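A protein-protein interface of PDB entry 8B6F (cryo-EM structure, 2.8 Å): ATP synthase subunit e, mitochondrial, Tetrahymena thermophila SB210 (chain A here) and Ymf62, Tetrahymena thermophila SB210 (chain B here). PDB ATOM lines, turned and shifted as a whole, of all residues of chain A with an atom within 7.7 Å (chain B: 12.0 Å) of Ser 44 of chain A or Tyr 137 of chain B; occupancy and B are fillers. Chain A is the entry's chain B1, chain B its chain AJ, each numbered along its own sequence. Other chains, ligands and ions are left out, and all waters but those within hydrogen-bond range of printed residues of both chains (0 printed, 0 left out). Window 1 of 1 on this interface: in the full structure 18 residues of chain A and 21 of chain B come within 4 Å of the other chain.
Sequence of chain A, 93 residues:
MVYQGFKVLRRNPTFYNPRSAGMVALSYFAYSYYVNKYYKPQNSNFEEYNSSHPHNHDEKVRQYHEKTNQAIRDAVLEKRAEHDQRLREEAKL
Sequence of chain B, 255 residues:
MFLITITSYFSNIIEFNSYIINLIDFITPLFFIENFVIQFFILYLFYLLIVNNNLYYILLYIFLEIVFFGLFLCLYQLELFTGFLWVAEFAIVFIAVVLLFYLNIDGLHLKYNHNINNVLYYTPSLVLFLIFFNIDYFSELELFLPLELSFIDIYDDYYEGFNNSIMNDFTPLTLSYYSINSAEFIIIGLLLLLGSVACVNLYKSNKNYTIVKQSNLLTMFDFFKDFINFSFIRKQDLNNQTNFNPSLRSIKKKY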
ATOM      1  N   TYR A  38      19.580  18.700  -7.746  1.00  0.00           N
ATOM      2  CA  TYR A  38      19.821  17.597  -6.825  1.00  0.00           C
ATOM      3  C   TYR A  38      21.186  16.948  -6.993  1.00  0.00           C
ATOM      4  O   TYR A  38      21.899  16.751  -6.004  1.00  0.00           O
ATOM      5  CB  TYR A  38      18.725  16.534  -6.988  1.00  0.00           C
ATOM      6  CG  TYR A  38      19.070  15.213  -6.343  1.00  0.00           C
ATOM      7  CD1 TYR A  38      18.961  15.038  -4.970  1.00  0.00           C
ATOM      8  CD2 TYR A  38      19.504  14.140  -7.108  1.00  0.00           C
ATOM      9  CE1 TYR A  38      19.277  13.831  -4.379  1.00  0.00           C
ATOM     10  CE2 TYR A  38      19.822  12.929  -6.525  1.00  0.00           C
ATOM     11  CZ  TYR A  38      19.708  12.782  -5.162  1.00  0.00           C
ATOM     12  OH  TYR A  38      20.024  11.577  -4.580  1.00  0.00           O
ATOM     13  N   TYR A  39      21.582  16.610  -8.220  1.00  0.00           N
ATOM     14  CA  TYR A  39      22.690  15.676  -8.390  1.00  0.00           C
ATOM     15  C   TYR A  39      24.036  16.381  -8.282  1.00  0.00           C
ATOM     16  O   TYR A  39      24.887  15.998  -7.473  1.00  0.00           O
ATOM     17  CB  TYR A  39      22.565  14.946  -9.728  1.00  0.00           C
ATOM     18  CG  TYR A  39      23.377  13.674  -9.793  1.00  0.00           C
ATOM     19  CD1 TYR A  39      23.040  12.569  -9.021  1.00  0.00           C
ATOM     20  CD2 TYR A  39      24.475  13.573 -10.634  1.00  0.00           C
ATOM     21  CE1 TYR A  39      23.780  11.403  -9.080  1.00  0.00           C
ATOM     22  CE2 TYR A  39      25.219  12.413 -10.699  1.00  0.00           C
ATOM     23  CZ  TYR A  39      24.868  11.333  -9.923  1.00  0.00           C
ATOM     24  OH  TYR A  39      25.614  10.181  -9.994  1.00  0.00           O
ATOM     25  N   LYS A  40      24.248  17.415  -9.093  1.00  0.00           N
ATOM     26  CA  LYS A  40      25.513  18.140  -9.027  1.00  0.00           C
ATOM     27  C   LYS A  40      25.755  18.764  -7.660  1.00  0.00           C
ATOM     28  O   LYS A  40      26.885  18.648  -7.153  1.00  0.00           O
ATOM     29  CB  LYS A  40      25.566  19.196 -10.138  1.00  0.00           C
ATOM     30  CG  LYS A  40      26.826  20.046 -10.106  1.00  0.00           C
ATOM     31  CD  LYS A  40      27.090  20.715 -11.445  1.00  0.00           C
ATOM     32  CE  LYS A  40      25.949  21.628 -11.854  1.00  0.00           C
ATOM     33  NZ  LYS A  40      26.252  22.347 -13.123  1.00  0.00           N
ATOM     34  N   PRO A  41      24.784  19.419  -7.016  1.00  0.00           N
ATOM     35  CA  PRO A  41      25.036  19.916  -5.652  1.00  0.00           C
ATOM     36  C   PRO A  41      25.447  18.823  -4.684  1.00  0.00           C
ATOM     37  O   PRO A  41      26.298  19.053  -3.817  1.00  0.00           O
ATOM     38  CB  PRO A  41      23.695  20.553  -5.258  1.00  0.00           C
ATOM     39  CG  PRO A  41      23.040  20.885  -6.540  1.00  0.00           C
ATOM     40  CD  PRO A  41      23.457  19.822  -7.509  1.00  0.00           C
ATOM     41  N   GLN A  42      24.857  17.632  -4.804  1.00  0.00           N
ATOM     42  CA  GLN A  42      25.221  16.530  -3.921  1.00  0.00           C
ATOM     43  C   GLN A  42      26.690  16.164  -4.085  1.00  0.00           C
ATOM     44  O   GLN A  42      27.410  15.972  -3.098  1.00  0.00           O
ATOM     45  CB  GLN A  42      24.330  15.321  -4.207  1.00  0.00           C
ATOM     46  CG  GLN A  42      24.627  14.102  -3.346  1.00  0.00           C
ATOM     47  CD  GLN A  42      24.008  12.836  -3.902  1.00  0.00           C
ATOM     48  OE1 GLN A  42      23.147  12.885  -4.779  1.00  0.00           O
ATOM     49  NE2 GLN A  42      24.452  11.689  -3.398  1.00  0.00           N
ATOM     50  N   ASN A  43      27.155  16.059  -5.333  1.00  0.00           N
ATOM     51  CA  ASN A  43      28.550  15.708  -5.573  1.00  0.00           C
ATOM     52  C   ASN A  43      29.487  16.824  -5.132  1.00  0.00           C
ATOM     53  O   ASN A  43      30.558  16.559  -4.574  1.00  0.00           O
ATOM     54  CB  ASN A  43      28.762  15.388  -7.052  1.00  0.00           C
ATOM     55  CG  ASN A  43      27.963  14.187  -7.505  1.00  0.00           C
ATOM     56  OD1 ASN A  43      27.626  13.316  -6.706  1.00  0.00           O
ATOM     57  ND2 ASN A  43      27.658  14.132  -8.796  1.00  0.00           N
ATOM     58  N   SER A  44      29.106  18.079  -5.372  1.00  0.00           N
ATOM     59  CA  SER A  44      29.947  19.191  -4.948  1.00  0.00           C
ATOM     60  C   SER A  44      30.101  19.211  -3.433  1.00  0.00           C
ATOM     61  O   SER A  44      31.203  19.426  -2.916  1.00  0.00           O
ATOM     62  CB  SER A  44      29.364  20.510  -5.451  1.00  0.00           C
ATOM     63  OG  SER A  44      28.090  20.756  -4.882  1.00  0.00           O
ATOM     64  N   ASN A  45      29.008  18.981  -2.706  1.00  0.00           N
ATOM     65  CA  ASN A  45      29.036  18.892  -1.249  1.00  0.00           C
ATOM     66  C   ASN A  45      29.561  20.192  -0.635  1.00  0.00           C
ATOM     67  O   ASN A  45      30.535  20.213   0.117  1.00  0.00           O
ATOM     68  CB  ASN A  45      29.873  17.690  -0.806  1.00  0.00           C
ATOM     69  CG  ASN A  45      29.817  17.454   0.688  1.00  0.00           C
ATOM     70  OD1 ASN A  45      28.897  17.910   1.366  1.00  0.00           O
ATOM     71  ND2 ASN A  45      30.802  16.735   1.210  1.00  0.00           N
ATOM     72  N   PHE A  46      28.885  21.289  -0.977  1.00  0.00           N
ATOM     73  CA  PHE A  46      29.238  22.613  -0.485  1.00  0.00           C
ATOM     74  C   PHE A  46      28.320  23.107   0.624  1.00  0.00           C
ATOM     75  O   PHE A  46      28.568  24.184   1.174  1.00  0.00           O
ATOM     76  CB  PHE A  46      29.216  23.629  -1.635  1.00  0.00           C
ATOM     77  CG  PHE A  46      30.262  23.393  -2.691  1.00  0.00           C
ATOM     78  CD1 PHE A  46      31.384  22.620  -2.435  1.00  0.00           C
ATOM     79  CD2 PHE A  46      30.123  23.962  -3.946  1.00  0.00           C
ATOM     80  CE1 PHE A  46      32.340  22.416  -3.411  1.00  0.00           C
ATOM     81  CE2 PHE A  46      31.074  23.761  -4.924  1.00  0.00           C
ATOM     82  CZ  PHE A  46      32.184  22.987  -4.657  1.00  0.00           C
ATOM     83  N   GLU A  47      27.268  22.359   0.965  1.00  0.00           N
ATOM     84  CA  GLU A  47      26.321  22.849   1.962  1.00  0.00           C
ATOM     85  C   GLU A  47      26.988  23.035   3.318  1.00  0.00           C
ATOM     86  O   GLU A  47      26.762  24.045   3.995  1.00  0.00           O
ATOM     87  CB  GLU A  47      25.133  21.894   2.080  1.00  0.00           C
ATOM     88  CG  GLU A  47      24.143  22.299   3.167  1.00  0.00           C
ATOM     89  CD  GLU A  47      22.864  21.485   3.138  1.00  0.00           C
ATOM     90  OE1 GLU A  47      22.627  20.777   2.138  1.00  0.00           O
ATOM     91  OE2 GLU A  47      22.094  21.556   4.120  1.00  0.00           O
ATOM     92  N   TYR A  49      30.388  23.051   3.812  1.00  0.00           N
ATOM     93  CA  TYR A  49      31.805  23.301   3.588  1.00  0.00           C
ATOM     94  C   TYR A  49      32.354  24.231   4.662  1.00  0.00           C
ATOM     95  O   TYR A  49      31.786  25.292   4.933  1.00  0.00           O
ATOM     96  CB  TYR A  49      32.013  23.908   2.200  1.00  0.00           C
ATOM     97  CG  TYR A  49      33.452  23.909   1.743  1.00  0.00           C
ATOM     98  CD1 TYR A  49      33.992  22.811   1.088  1.00  0.00           C
ATOM     99  CD2 TYR A  49      34.268  25.009   1.963  1.00  0.00           C
ATOM    100  CE1 TYR A  49      35.307  22.808   0.667  1.00  0.00           C
ATOM    101  CE2 TYR A  49      35.583  25.017   1.546  1.00  0.00           C
ATOM    102  CZ  TYR A  49      36.097  23.913   0.899  1.00  0.00           C
ATOM    103  OH  TYR A  49      37.408  23.916   0.482  1.00  0.00           O
ATOM    104  N   GLU A  59      32.831  15.769   4.809  1.00  0.00           N
ATOM    105  CA  GLU A  59      33.338  17.057   5.268  1.00  0.00           C
ATOM    106  C   GLU A  59      34.226  16.896   6.495  1.00  0.00           C
ATOM    107  O   GLU A  59      35.258  17.566   6.609  1.00  0.00           O
ATOM    108  CB  GLU A  59      32.175  18.001   5.568  1.00  0.00           C
ATOM    109  CG  GLU A  59      32.603  19.363   6.097  1.00  0.00           C
ATOM    110  CD  GLU A  59      33.533  20.099   5.153  1.00  0.00           C
ATOM    111  OE1 GLU A  59      33.569  19.749   3.955  1.00  0.00           O
ATOM    112  OE2 GLU A  59      34.231  21.027   5.609  1.00  0.00           O
ATOM    113  N   ARG A  62      37.532  15.705   5.277  1.00  0.00           N
ATOM    114  CA  ARG A  62      38.267  16.778   4.616  1.00  0.00           C
ATOM    115  C   ARG A  62      38.891  17.720   5.634  1.00  0.00           C
ATOM    116  O   ARG A  62      40.056  18.110   5.497  1.00  0.00           O
ATOM    117  CB  ARG A  62      37.340  17.545   3.675  1.00  0.00           C
ATOM    118  CG  ARG A  62      38.067  18.516   2.757  1.00  0.00           C
ATOM    119  CD  ARG A  62      37.101  19.456   2.060  1.00  0.00           C
ATOM    120  NE  ARG A  62      36.406  20.311   3.014  1.00  0.00           N
ATOM    121  CZ  ARG A  62      36.934  21.388   3.580  1.00  0.00           C
ATOM    122  NH1 ARG A  62      38.173  21.770   3.316  1.00  0.00           N
ATOM    123  NH2 ARG A  62      36.204  22.096   4.435  1.00  0.00           N
ATOM    124  N   PHE B 132      22.879   8.123 -13.298  1.00  0.00           N
ATOM    125  CA  PHE B 132      24.137   7.921 -12.593  1.00  0.00           C
ATOM    126  C   PHE B 132      25.331   8.615 -13.240  1.00  0.00           C
ATOM    127  O   PHE B 132      26.462   8.395 -12.800  1.00  0.00           O
ATOM    128  CB  PHE B 132      24.424   6.427 -12.474  1.00  0.00           C
ATOM    129  CG  PHE B 132      23.476   5.717 -11.570  1.00  0.00           C
ATOM    130  CD1 PHE B 132      23.486   5.967 -10.216  1.00  0.00           C
ATOM    131  CD2 PHE B 132      22.574   4.795 -12.075  1.00  0.00           C
ATOM    132  CE1 PHE B 132      22.613   5.326  -9.381  1.00  0.00           C
ATOM    133  CE2 PHE B 132      21.693   4.144 -11.240  1.00  0.00           C
ATOM    134  CZ  PHE B 132      21.715   4.407  -9.888  1.00  0.00           C
ATOM    135  N   PHE B 133      25.119   9.454 -14.250  1.00  0.00           N
ATOM    136  CA  PHE B 133      26.221  10.079 -14.972  1.00  0.00           C
ATOM    137  C   PHE B 133      26.171  11.587 -14.787  1.00  0.00           C
ATOM    138  O   PHE B 133      25.220  12.241 -15.229  1.00  0.00           O
ATOM    139  CB  PHE B 133      26.178   9.732 -16.460  1.00  0.00           C
ATOM    140  CG  PHE B 133      27.274  10.375 -17.257  1.00  0.00           C
ATOM    141  CD1 PHE B 133      28.542   9.823 -17.288  1.00  0.00           C
ATOM    142  CD2 PHE B 133      27.034  11.538 -17.969  1.00  0.00           C
ATOM    143  CE1 PHE B 133      29.549  10.419 -18.017  1.00  0.00           C
ATOM    144  CE2 PHE B 133      28.038  12.138 -18.700  1.00  0.00           C
ATOM    145  CZ  PHE B 133      29.297  11.577 -18.724  1.00  0.00           C
ATOM    146  N   ASN B 134      27.199  12.132 -14.141  1.00  0.00           N
ATOM    147  CA  ASN B 134      27.431  13.573 -14.139  1.00  0.00           C
ATOM    148  C   ASN B 134      28.896  13.788 -13.790  1.00  0.00           C
ATOM    149  O   ASN B 134      29.309  13.498 -12.663  1.00  0.00           O
ATOM    150  CB  ASN B 134      26.518  14.283 -13.151  1.00  0.00           C
ATOM    151  CG  ASN B 134      26.644  15.790 -13.228  1.00  0.00           C
ATOM    152  OD1 ASN B 134      27.341  16.408 -12.424  1.00  0.00           O
ATOM    153  ND2 ASN B 134      25.977  16.390 -14.207  1.00  0.00           N
ATOM    154  N   ILE B 135      29.674  14.288 -14.748  1.00  0.00           N
ATOM    155  CA  ILE B 135      31.085  14.551 -14.498  1.00  0.00           C
ATOM    156  C   ILE B 135      31.338  15.993 -14.078  1.00  0.00           C
ATOM    157  O   ILE B 135      32.356  16.269 -13.430  1.00  0.00           O
ATOM    158  CB  ILE B 135      31.936  14.216 -15.735  1.00  0.00           C
ATOM    159  CG1 ILE B 135      31.615  12.808 -16.244  1.00  0.00           C
ATOM    160  CG2 ILE B 135      33.411  14.311 -15.388  1.00  0.00           C
ATOM    161  CD1 ILE B 135      32.340  12.430 -17.523  1.00  0.00           C
ATOM    162  N   ASP B 136      30.444  16.916 -14.418  1.00  0.00           N
ATOM    163  CA  ASP B 136      30.607  18.301 -13.995  1.00  0.00           C
ATOM    164  C   ASP B 136      30.619  18.377 -12.475  1.00  0.00           C
ATOM    165  O   ASP B 136      29.625  18.052 -11.820  1.00  0.00           O
ATOM    166  CB  ASP B 136      29.481  19.153 -14.573  1.00  0.00           C
ATOM    167  CG  ASP B 136      29.663  20.626 -14.292  1.00  0.00           C
ATOM    168  OD1 ASP B 136      30.740  21.162 -14.619  1.00  0.00           O
ATOM    169  OD2 ASP B 136      28.728  21.251 -13.755  1.00  0.00           O
ATOM    170  N   TYR B 137      31.749  18.813 -11.916  1.00  0.00           N
ATOM    171  CA  TYR B 137      31.931  18.778 -10.469  1.00  0.00           C
ATOM    172  C   TYR B 137      31.240  19.956  -9.791  1.00  0.00           C
ATOM    173  O   TYR B 137      30.295  19.772  -9.016  1.00  0.00           O
ATOM    174  CB  TYR B 137      33.430  18.767 -10.142  1.00  0.00           C
ATOM    175  CG  TYR B 137      33.778  18.441  -8.701  1.00  0.00           C
ATOM    176  CD1 TYR B 137      32.791  18.184  -7.757  1.00  0.00           C
ATOM    177  CD2 TYR B 137      35.102  18.397  -8.288  1.00  0.00           C
ATOM    178  CE1 TYR B 137      33.115  17.891  -6.447  1.00  0.00           C
ATOM    179  CE2 TYR B 137      35.435  18.104  -6.981  1.00  0.00           C
ATOM    180  CZ  TYR B 137      34.437  17.852  -6.064  1.00  0.00           C
ATOM    181  OH  TYR B 137      34.763  17.560  -4.761  1.00  0.00           O
ATOM    182  N   PHE B 138      31.700  21.178 -10.071  1.00  0.00           N
ATOM    183  CA  PHE B 138      31.190  22.349  -9.370  1.00  0.00           C
ATOM    184  C   PHE B 138      30.951  23.540 -10.290  1.00  0.00           C
ATOM    185  O   PHE B 138      30.749  24.654  -9.791  1.00  0.00           O
ATOM    186  CB  PHE B 138      32.151  22.754  -8.244  1.00  0.00           C
ATOM    187  CG  PHE B 138      33.599  22.661  -8.621  1.00  0.00           C
ATOM    188  CD1 PHE B 138      34.157  23.566  -9.507  1.00  0.00           C
ATOM    189  CD2 PHE B 138      34.407  21.675  -8.081  1.00  0.00           C
ATOM    190  CE1 PHE B 138      35.491  23.485  -9.853  1.00  0.00           C
ATOM    191  CE2 PHE B 138      35.741  21.587  -8.422  1.00  0.00           C
ATOM    192  CZ  PHE B 138      36.284  22.494  -9.309  1.00  0.00           C
ATOM    193  N   SER B 139      30.961  23.352 -11.606  1.00  0.00           N
ATOM    194  CA  SER B 139      30.711  24.463 -12.513  1.00  0.00           C
ATOM    195  C   SER B 139      29.342  25.068 -12.236  1.00  0.00           C
ATOM    196  O   SER B 139      28.368  24.356 -11.978  1.00  0.00           O
ATOM    197  CB  SER B 139      30.790  23.995 -13.964  1.00  0.00           C
ATOM    198  OG  SER B 139      30.718  25.098 -14.847  1.00  0.00           O
ATOM    199  N   GLU B 140      29.271  26.395 -12.287  1.00  0.00           N
ATOM    200  CA  GLU B 140      28.068  27.131 -11.933  1.00  0.00           C
ATOM    201  C   GLU B 140      27.481  27.803 -13.166  1.00  0.00           C
ATOM    202  O   GLU B 140      28.210  28.371 -13.983  1.00  0.00           O
ATOM    203  CB  GLU B 140      28.372  28.181 -10.862  1.00  0.00           C
ATOM    204  CG  GLU B 140      29.238  29.326 -11.353  1.00  0.00           C
ATOM    205  CD  GLU B 140      29.736  30.202 -10.223  1.00  0.00           C
ATOM    206  OE1 GLU B 140      29.727  29.739  -9.064  1.00  0.00           O
ATOM    207  OE2 GLU B 140      30.132  31.355 -10.492  1.00  0.00           O
ATOM    208  N   LEU B 141      26.159  27.728 -13.291  1.00  0.00           N
ATOM    209  CA  LEU B 141      25.469  28.370 -14.398  1.00  0.00           C
ATOM    210  C   LEU B 141      25.565  29.886 -14.291  1.00  0.00           C
ATOM    211  O   LEU B 141      25.744  30.446 -13.208  1.00  0.00           O
ATOM    212  CB  LEU B 141      23.994  27.966 -14.418  1.00  0.00           C
ATOM    213  CG  LEU B 141      23.636  26.602 -15.001  1.00  0.00           C
ATOM    214  CD1 LEU B 141      22.199  26.251 -14.666  1.00  0.00           C
ATOM    215  CD2 LEU B 141      23.848  26.600 -16.502  1.00  0.00           C
ATOM    216  N   PHE B 144      23.642  32.195 -11.683  1.00  0.00           N
ATOM    217  CA  PHE B 144      23.803  31.610 -10.358  1.00  0.00           C
ATOM    218  C   PHE B 144      24.019  32.695  -9.313  1.00  0.00           C
ATOM    219  O   PHE B 144      23.440  32.643  -8.222  1.00  0.00           O
ATOM    220  CB  PHE B 144      24.970  30.623 -10.369  1.00  0.00           C
ATOM    221  CG  PHE B 144      25.254  30.000  -9.036  1.00  0.00           C
ATOM    222  CD1 PHE B 144      24.544  28.893  -8.608  1.00  0.00           C
ATOM    223  CD2 PHE B 144      26.244  30.514  -8.216  1.00  0.00           C
ATOM    224  CE1 PHE B 144      24.809  28.316  -7.384  1.00  0.00           C
ATOM    225  CE2 PHE B 144      26.515  29.941  -6.993  1.00  0.00           C
ATOM    226  CZ  PHE B 144      25.797  28.840  -6.575  1.00  0.00           C
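The backbone carbonyl oxygen of Phe 132 of chain B lies within hydrogen-bond range of the side-chain hydroxyl of Tyr 39 of chain A (3.4 Å). The side-chain amino group of Lys 40 of chain A lies within salt-bridge range of the side-chain carboxylate of Asp 136 of chain B (2.8 Å). The side-chain amino group (NZ) of Lys 40 of chain A sits at hydrogen-bond distance from the backbone carbonyl oxygen (O) of Ser 139 of chain B.
The side-chain amide oxygen of Asn 134 of chain B sits close to the backbone carbonyl oxygen of Asp 136 of chain B. OG of Ser 44 of chain A sits at hydrogen-bond distance from O of Lys 40 of chain A (3.3 Å). O of Pro 41 of chain A sits at hydrogen-bond distance from OG of Ser 44 of chain A.
Among the printed residues, merely in contact across the chains: Tyr 39 of chain A with Asn 134 of chain B, Asn 43 of chain A with Tyr 137 of chain B, Phe 46 of chain A with Phe 138 of chain B, Lys 40 of chain A with Tyr 137 of chain B and Ser 44 of chain A with Tyr 137 of chain B.
Of chain A, only Lys 40 (3.6 Å), Asn 43 (3.4 Å) and Ser 44 (3.7 Å) come within 4 Å of Tyr 137 of chain B. No residue of chain B comes within 4 Å of Pro 41 of chain A. Of chain B, only Phe 138 (3.6 Å) comes within 4 Å of Phe 46 of chain A. Printed residues of chain A within 4 Å of Asn 134 of chain B: Tyr 39 (3.3 Å). Of the printed residues of chain A, Ser 139 of chain B touches Lys 40 (3.1 Å). Gln 42 of chain A touches none of the printed residues of chain B. Phe 144 of chain B touches none of the printed residues of chain A. The nearest residue of chain B that does not touch Ser 44 of chain A is Phe 138 of chain B (4.5 Å).
Of the 11 printed residues of chain B, 6 touch a printed residue of chain A. Hydrophobic or aromatic side chains of chain B that line the printed part of chain A: Tyr 137 and Phe 138. Among the printed residues, 8 pairs touch across the chains.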
